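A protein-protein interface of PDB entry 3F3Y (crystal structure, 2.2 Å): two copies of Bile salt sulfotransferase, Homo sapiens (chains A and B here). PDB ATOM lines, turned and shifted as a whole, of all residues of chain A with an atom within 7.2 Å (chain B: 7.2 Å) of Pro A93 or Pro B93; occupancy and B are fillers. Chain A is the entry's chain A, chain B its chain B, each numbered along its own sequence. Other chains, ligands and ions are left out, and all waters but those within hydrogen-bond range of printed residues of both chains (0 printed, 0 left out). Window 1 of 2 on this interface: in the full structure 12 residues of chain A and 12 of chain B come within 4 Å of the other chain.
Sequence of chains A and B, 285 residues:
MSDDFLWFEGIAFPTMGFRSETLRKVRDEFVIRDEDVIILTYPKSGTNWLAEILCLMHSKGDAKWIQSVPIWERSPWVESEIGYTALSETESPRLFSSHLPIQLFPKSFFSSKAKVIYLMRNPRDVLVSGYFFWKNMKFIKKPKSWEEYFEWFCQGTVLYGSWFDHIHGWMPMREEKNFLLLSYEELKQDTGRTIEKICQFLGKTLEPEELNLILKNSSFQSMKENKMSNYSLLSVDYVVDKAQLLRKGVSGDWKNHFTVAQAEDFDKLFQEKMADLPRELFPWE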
ATOM      1  N   ARG A  33      20.305 -19.173   6.415  1.00  0.00           N
ATOM      2  CA  ARG A  33      19.330 -18.142   6.145  1.00  0.00           C
ATOM      3  C   ARG A  33      20.095 -16.967   5.595  1.00  0.00           C
ATOM      4  O   ARG A  33      21.263 -16.825   5.879  1.00  0.00           O
ATOM      5  CB  ARG A  33      18.559 -17.763   7.416  1.00  0.00           C
ATOM      6  CG  ARG A  33      18.027 -18.992   8.222  1.00  0.00           C
ATOM      7  CD  ARG A  33      17.370 -18.552   9.526  1.00  0.00           C
ATOM      8  NE  ARG A  33      17.051 -19.702  10.416  1.00  0.00           N
ATOM      9  CZ  ARG A  33      16.848 -19.609  11.712  1.00  0.00           C
ATOM     10  NH1 ARG A  33      16.928 -18.429  12.310  1.00  0.00           N
ATOM     11  NH2 ARG A  33      16.597 -20.705  12.436  1.00  0.00           N
ATOM     12  N   GLU A  35      19.949 -14.044   6.448  1.00  0.00           N
ATOM     13  CA  GLU A  35      20.161 -13.099   7.554  1.00  0.00           C
ATOM     14  C   GLU A  35      21.349 -13.483   8.499  1.00  0.00           C
ATOM     15  O   GLU A  35      21.790 -12.654   9.297  1.00  0.00           O
ATOM     16  CB  GLU A  35      18.877 -12.964   8.412  1.00  0.00           C
ATOM     17  CG  GLU A  35      17.737 -12.171   7.772  1.00  0.00           C
ATOM     18  CD  GLU A  35      17.128 -12.880   6.541  1.00  0.00           C
ATOM     19  OE1 GLU A  35      16.925 -12.207   5.482  1.00  0.00           O
ATOM     20  OE2 GLU A  35      16.888 -14.110   6.624  1.00  0.00           O
ATOM     21  N   ASP A  36      21.791 -14.753   8.431  1.00  0.00           N
ATOM     22  CA  ASP A  36      22.965 -15.244   9.153  1.00  0.00           C
ATOM     23  C   ASP A  36      24.214 -14.403   8.918  1.00  0.00           C
ATOM     24  O   ASP A  36      24.461 -13.935   7.813  1.00  0.00           O
ATOM     25  CB  ASP A  36      23.265 -16.687   8.780  1.00  0.00           C
ATOM     26  CG  ASP A  36      22.188 -17.642   9.220  1.00  0.00           C
ATOM     27  OD1 ASP A  36      22.186 -18.771   8.686  1.00  0.00           O
ATOM     28  OD2 ASP A  36      21.333 -17.287  10.081  1.00  0.00           O
ATOM     29  N   VAL A  37      24.976 -14.207  10.002  1.00  0.00           N
ATOM     30  CA  VAL A  37      26.337 -13.680   9.949  1.00  0.00           C
ATOM     31  C   VAL A  37      27.241 -14.771  10.485  1.00  0.00           C
ATOM     32  O   VAL A  37      27.045 -15.284  11.619  1.00  0.00           O
ATOM     33  CB  VAL A  37      26.478 -12.378  10.775  1.00  0.00           C
ATOM     34  CG1 VAL A  37      27.900 -11.775  10.644  1.00  0.00           C
ATOM     35  CG2 VAL A  37      25.468 -11.373  10.298  1.00  0.00           C
ATOM     36  N   HIS A  58      26.335  -5.340  17.457  1.00  0.00           N
ATOM     37  CA  HIS A  58      24.947  -5.641  17.520  1.00  0.00           C
ATOM     38  C   HIS A  58      24.239  -4.944  18.661  1.00  0.00           C
ATOM     39  O   HIS A  58      23.077  -4.620  18.547  1.00  0.00           O
ATOM     40  CB  HIS A  58      24.764  -7.136  17.680  1.00  0.00           C
ATOM     41  CG  HIS A  58      23.340  -7.560  17.611  1.00  0.00           C
ATOM     42  ND1 HIS A  58      22.564  -7.366  16.489  1.00  0.00           N
ATOM     43  CD2 HIS A  58      22.526  -8.112  18.543  1.00  0.00           C
ATOM     44  CE1 HIS A  58      21.339  -7.798  16.723  1.00  0.00           C
ATOM     45  NE2 HIS A  58      21.290  -8.256  17.965  1.00  0.00           N
ATOM     46  N   THR A  90      17.126 -21.315  16.701  1.00  0.00           N
ATOM     47  CA  THR A  90      17.446 -19.935  16.998  1.00  0.00           C
ATOM     48  C   THR A  90      16.815 -19.031  15.941  1.00  0.00           C
ATOM     49  O   THR A  90      16.896 -19.298  14.711  1.00  0.00           O
ATOM     50  CB  THR A  90      19.036 -19.721  17.114  1.00  0.00           C
ATOM     51  OG1 THR A  90      19.551 -20.573  18.145  1.00  0.00           O
ATOM     52  CG2 THR A  90      19.397 -18.299  17.490  1.00  0.00           C
ATOM     53  N   GLU A  91      16.168 -17.967  16.422  1.00  0.00           N
ATOM     54  CA  GLU A  91      15.568 -16.972  15.563  1.00  0.00           C
ATOM     55  C   GLU A  91      16.667 -16.096  14.961  1.00  0.00           C
ATOM     56  O   GLU A  91      17.723 -15.929  15.550  1.00  0.00           O
ATOM     57  CB  GLU A  91      14.618 -16.087  16.372  1.00  0.00           C
ATOM     58  CG  GLU A  91      13.580 -16.814  17.173  1.00  0.00           C
ATOM     59  CD  GLU A  91      12.509 -15.871  17.689  1.00  0.00           C
ATOM     60  OE1 GLU A  91      12.077 -14.979  16.921  1.00  0.00           O
ATOM     61  OE2 GLU A  91      12.109 -16.012  18.862  1.00  0.00           O
ATOM     62  N   SER A  92      16.409 -15.546  13.784  1.00  0.00           N
ATOM     63  CA  SER A  92      17.303 -14.591  13.175  1.00  0.00           C
ATOM     64  C   SER A  92      17.334 -13.269  13.945  1.00  0.00           C
ATOM     65  O   SER A  92      16.376 -12.908  14.578  1.00  0.00           O
ATOM     66  CB  SER A  92      16.870 -14.364  11.736  1.00  0.00           C
ATOM     67  OG  SER A  92      16.954 -15.581  10.985  1.00  0.00           O
ATOM     68  N   PRO A  93      18.433 -12.514  13.843  1.00  0.00           N
ATOM     69  CA  PRO A  93      19.632 -12.804  13.011  1.00  0.00           C
ATOM     70  C   PRO A  93      20.571 -13.649  13.810  1.00  0.00           C
ATOM     71  O   PRO A  93      20.822 -13.323  14.928  1.00  0.00           O
ATOM     72  CB  PRO A  93      20.252 -11.438  12.782  1.00  0.00           C
ATOM     73  CG  PRO A  93      19.618 -10.501  13.849  1.00  0.00           C
ATOM     74  CD  PRO A  93      18.570 -11.266  14.609  1.00  0.00           C
ATOM     75  N   ARG A  94      21.044 -14.749  13.235  1.00  0.00           N
ATOM     76  CA  ARG A  94      21.954 -15.638  13.905  1.00  0.00           C
ATOM     77  C   ARG A  94      23.361 -15.251  13.625  1.00  0.00           C
ATOM     78  O   ARG A  94      23.746 -15.040  12.461  1.00  0.00           O
ATOM     79  CB  ARG A  94      21.764 -17.084  13.430  1.00  0.00           C
ATOM     80  CG  ARG A  94      20.333 -17.522  13.332  1.00  0.00           C
ATOM     81  CD  ARG A  94      20.230 -19.005  13.104  1.00  0.00           C
ATOM     82  NE  ARG A  94      20.562 -19.360  11.751  1.00  0.00           N
ATOM     83  CZ  ARG A  94      20.435 -20.597  11.253  1.00  0.00           C
ATOM     84  NH1 ARG A  94      19.996 -21.615  12.010  1.00  0.00           N
ATOM     85  NH2 ARG A  94      20.788 -20.826  10.028  1.00  0.00           N
ATOM     86  N   LEU A  95      24.157 -15.213  14.686  1.00  0.00           N
ATOM     87  CA  LEU A  95      25.600 -15.205  14.572  1.00  0.00           C
ATOM     88  C   LEU A  95      26.102 -16.566  14.922  1.00  0.00           C
ATOM     89  O   LEU A  95      25.630 -17.188  15.933  1.00  0.00           O
ATOM     90  CB  LEU A  95      26.210 -14.144  15.508  1.00  0.00           C
ATOM     91  CG  LEU A  95      27.728 -13.911  15.471  1.00  0.00           C
ATOM     92  CD1 LEU A  95      28.146 -13.454  14.085  1.00  0.00           C
ATOM     93  CD2 LEU A  95      28.141 -12.906  16.524  1.00  0.00           C
ATOM     94  N   ARG B  33      15.409   1.717  20.880  1.00  0.00           N
ATOM     95  CA  ARG B  33      16.544   1.499  19.999  1.00  0.00           C
ATOM     96  C   ARG B  33      16.063   1.737  18.584  1.00  0.00           C
ATOM     97  O   ARG B  33      14.911   1.491  18.286  1.00  0.00           O
ATOM     98  CB  ARG B  33      17.071   0.059  20.144  1.00  0.00           C
ATOM     99  CG  ARG B  33      17.305  -0.413  21.625  1.00  0.00           C
ATOM    100  CD  ARG B  33      17.725  -1.899  21.681  1.00  0.00           C
ATOM    101  NE  ARG B  33      17.738  -2.385  23.058  1.00  0.00           N
ATOM    102  CZ  ARG B  33      17.686  -3.652  23.430  1.00  0.00           C
ATOM    103  NH1 ARG B  33      17.639  -4.606  22.527  1.00  0.00           N
ATOM    104  NH2 ARG B  33      17.654  -3.969  24.741  1.00  0.00           N
ATOM    105  N   GLU B  35      16.391  -0.084  16.210  1.00  0.00           N
ATOM    106  CA  GLU B  35      16.106  -1.394  15.604  1.00  0.00           C
ATOM    107  C   GLU B  35      14.729  -1.969  16.011  1.00  0.00           C
ATOM    108  O   GLU B  35      14.296  -3.026  15.526  1.00  0.00           O
ATOM    109  CB  GLU B  35      17.255  -2.378  15.868  1.00  0.00           C
ATOM    110  CG  GLU B  35      18.545  -2.051  15.010  1.00  0.00           C
ATOM    111  CD  GLU B  35      19.303  -0.784  15.496  1.00  0.00           C
ATOM    112  OE1 GLU B  35      19.869  -0.052  14.637  1.00  0.00           O
ATOM    113  OE2 GLU B  35      19.332  -0.517  16.733  1.00  0.00           O
ATOM    114  N   ASP B  36      14.018  -1.201  16.829  1.00  0.00           N
ATOM    115  CA  ASP B  36      12.728  -1.601  17.316  1.00  0.00           C
ATOM    116  C   ASP B  36      11.701  -1.535  16.240  1.00  0.00           C
ATOM    117  O   ASP B  36      11.767  -0.672  15.352  1.00  0.00           O
ATOM    118  CB  ASP B  36      12.306  -0.762  18.519  1.00  0.00           C
ATOM    119  CG  ASP B  36      13.112  -1.080  19.751  1.00  0.00           C
ATOM    120  OD1 ASP B  36      13.046  -0.313  20.739  1.00  0.00           O
ATOM    121  OD2 ASP B  36      13.850  -2.076  19.721  1.00  0.00           O
ATOM    122  N   VAL B  37      10.796  -2.514  16.287  1.00  0.00           N
ATOM    123  CA  VAL B  37       9.582  -2.525  15.523  1.00  0.00           C
ATOM    124  C   VAL B  37       8.454  -2.551  16.516  1.00  0.00           C
ATOM    125  O   VAL B  37       8.391  -3.450  17.427  1.00  0.00           O
ATOM    126  CB  VAL B  37       9.525  -3.745  14.593  1.00  0.00           C
ATOM    127  CG1 VAL B  37       8.156  -3.823  13.881  1.00  0.00           C
ATOM    128  CG2 VAL B  37      10.669  -3.658  13.548  1.00  0.00           C
ATOM    129  N   HIS B  58       9.255 -12.416  10.063  1.00  0.00           N
ATOM    130  CA  HIS B  58      10.574 -12.478  10.597  1.00  0.00           C
ATOM    131  C   HIS B  58      11.171 -13.853  10.362  1.00  0.00           C
ATOM    132  O   HIS B  58      12.352 -13.961  10.070  1.00  0.00           O
ATOM    133  CB  HIS B  58      10.539 -12.177  12.089  1.00  0.00           C
ATOM    134  CG  HIS B  58      11.891 -12.161  12.730  1.00  0.00           C
ATOM    135  ND1 HIS B  58      12.882 -11.273  12.354  1.00  0.00           N
ATOM    136  CD2 HIS B  58      12.424 -12.926  13.714  1.00  0.00           C
ATOM    137  CE1 HIS B  58      13.961 -11.489  13.080  1.00  0.00           C
ATOM    138  NE2 HIS B  58      13.707 -12.481  13.921  1.00  0.00           N
ATOM    139  N   THR B  90      16.102  -7.816  26.543  1.00  0.00           N
ATOM    140  CA  THR B  90      15.989  -8.471  25.254  1.00  0.00           C
ATOM    141  C   THR B  90      16.976  -7.865  24.266  1.00  0.00           C
ATOM    142  O   THR B  90      17.135  -6.646  24.195  1.00  0.00           O
ATOM    143  CB  THR B  90      14.505  -8.355  24.731  1.00  0.00           C
ATOM    144  OG1 THR B  90      13.634  -9.024  25.655  1.00  0.00           O
ATOM    145  CG2 THR B  90      14.324  -8.967  23.355  1.00  0.00           C
ATOM    146  N   GLU B  91      17.641  -8.729  23.497  1.00  0.00           N
ATOM    147  CA  GLU B  91      18.535  -8.287  22.419  1.00  0.00           C
ATOM    148  C   GLU B  91      17.711  -7.794  21.231  1.00  0.00           C
ATOM    149  O   GLU B  91      16.588  -8.228  21.049  1.00  0.00           O
ATOM    150  CB  GLU B  91      19.419  -9.453  21.944  1.00  0.00           C
ATOM    151  CG  GLU B  91      20.374  -9.979  22.957  1.00  0.00           C
ATOM    152  CD  GLU B  91      21.386 -10.932  22.361  1.00  0.00           C
ATOM    153  OE1 GLU B  91      22.147 -10.519  21.463  1.00  0.00           O
ATOM    154  OE2 GLU B  91      21.430 -12.092  22.803  1.00  0.00           O
ATOM    155  N   SER B  92      18.291  -6.924  20.409  1.00  0.00           N
ATOM    156  CA  SER B  92      17.687  -6.530  19.160  1.00  0.00           C
ATOM    157  C   SER B  92      17.656  -7.704  18.179  1.00  0.00           C
ATOM    158  O   SER B  92      18.403  -8.651  18.338  1.00  0.00           O
ATOM    159  CB  SER B  92      18.473  -5.365  18.543  1.00  0.00           C
ATOM    160  OG  SER B  92      18.268  -4.158  19.259  1.00  0.00           O
ATOM    161  N   PRO B  93      16.761  -7.660  17.175  1.00  0.00           N
ATOM    162  CA  PRO B  93      15.645  -6.708  16.982  1.00  0.00           C
ATOM    163  C   PRO B  93      14.466  -7.029  17.904  1.00  0.00           C
ATOM    164  O   PRO B  93      14.045  -8.157  17.971  1.00  0.00           O
ATOM    165  CB  PRO B  93      15.257  -6.918  15.529  1.00  0.00           C
ATOM    166  CG  PRO B  93      15.669  -8.352  15.236  1.00  0.00           C
ATOM    167  CD  PRO B  93      16.853  -8.640  16.084  1.00  0.00           C
ATOM    168  N   ARG B  94      13.982  -6.029  18.640  1.00  0.00           N
ATOM    169  CA  ARG B  94      12.833  -6.185  19.519  1.00  0.00           C
ATOM    170  C   ARG B  94      11.562  -5.922  18.768  1.00  0.00           C
ATOM    171  O   ARG B  94      11.478  -4.971  17.967  1.00  0.00           O
ATOM    172  CB  ARG B  94      12.938  -5.237  20.716  1.00  0.00           C
ATOM    173  CG  ARG B  94      14.133  -5.566  21.629  1.00  0.00           C
ATOM    174  CD  ARG B  94      14.170  -4.771  22.902  1.00  0.00           C
ATOM    175  NE  ARG B  94      14.132  -3.333  22.738  1.00  0.00           N
ATOM    176  CZ  ARG B  94      14.184  -2.480  23.769  1.00  0.00           C
ATOM    177  NH1 ARG B  94      14.288  -2.923  25.037  1.00  0.00           N
ATOM    178  NH2 ARG B  94      14.091  -1.207  23.550  1.00  0.00           N
ATOM    179  N   LEU B  95      10.586  -6.799  18.961  1.00  0.00           N
ATOM    180  CA  LEU B  95       9.244  -6.522  18.530  1.00  0.00           C
ATOM    181  C   LEU B  95       8.475  -6.337  19.761  1.00  0.00           C
ATOM    182  O   LEU B  95       8.620  -7.124  20.693  1.00  0.00           O
ATOM    183  CB  LEU B  95       8.675  -7.699  17.744  1.00  0.00           C
ATOM    184  CG  LEU B  95       7.213  -7.577  17.297  1.00  0.00           C
ATOM    185  CD1 LEU B  95       7.084  -6.450  16.204  1.00  0.00           C
ATOM    186  CD2 LEU B  95       6.674  -8.888  16.761  1.00  0.00           C
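NH1 of Arg A33 sits at hydrogen-bond distance from OG of Ser A92 (3.1 Å). The guanidinium group (NH1) of Arg B33 lies close to the side-chain hydroxyl (OG) of Ser B92, at 3.4 Å.
NE2 of His A58 sits at hydrogen-bond distance from O of Ser B92 (2.9 Å). The backbone carbonyl oxygen of Ser A92 sits at hydrogen-bond distance from a ring nitrogen (NE2) of His B58, 2.8 Å away.
Hydrophobic or aromatic side chains of chain A that line the printed part of chain B: His A58 and Pro A93. Of the 11 printed residues of chain B, 4 touch a printed residue of chain A. Printed residues of chain B that touch a printed residue of chain A: His B58, Glu B91, Ser B92 and Pro B93. Hydrophobic or aromatic side chains of chain B that line the printed part of chain A: His B58 and Pro B93.
His A58 touches Glu B91, and with the chains exchanged Glu A91 touches His B58. His A58 touches Ser B92, and with the chains exchanged Ser A92 touches His B58. Pro A93 touches its own counterpart, Pro B93. Positions printed for both chains: 33, 35, 36, 37, 58, 90, 91, 92, 93, 94 and 95.
Printed residues of chain B within 4 Å of His A58: Glu B91 and Ser B92. Of the printed residues of chain B, Glu A91 touches His B58 (3.8 Å). Printed residues of chain B within 4 Å of Ser A92: His B58. Pro A93 touches just one residue of chain B: Pro B93 (3.5 Å). Thr B90 touches none of the printed residues of chain A. Of chain A, only Pro A93 comes within 4 Å of Pro B93. Arg B94 touches none of the printed residues of chain A. The nearest residue of chain B that does not touch Pro A93 is Ser B92 (4.6 Å). The nearest residue of chain A that does not touch Pro B93 is Ser A92 (4.6 Å).
Among the printed residues, pairs that only touch across the chains: His A58 with Glu B91 (3.8 Å), Glu A91 with His B58 (3.8 Å) and Pro A93 with Pro B93 (3.5 Å).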
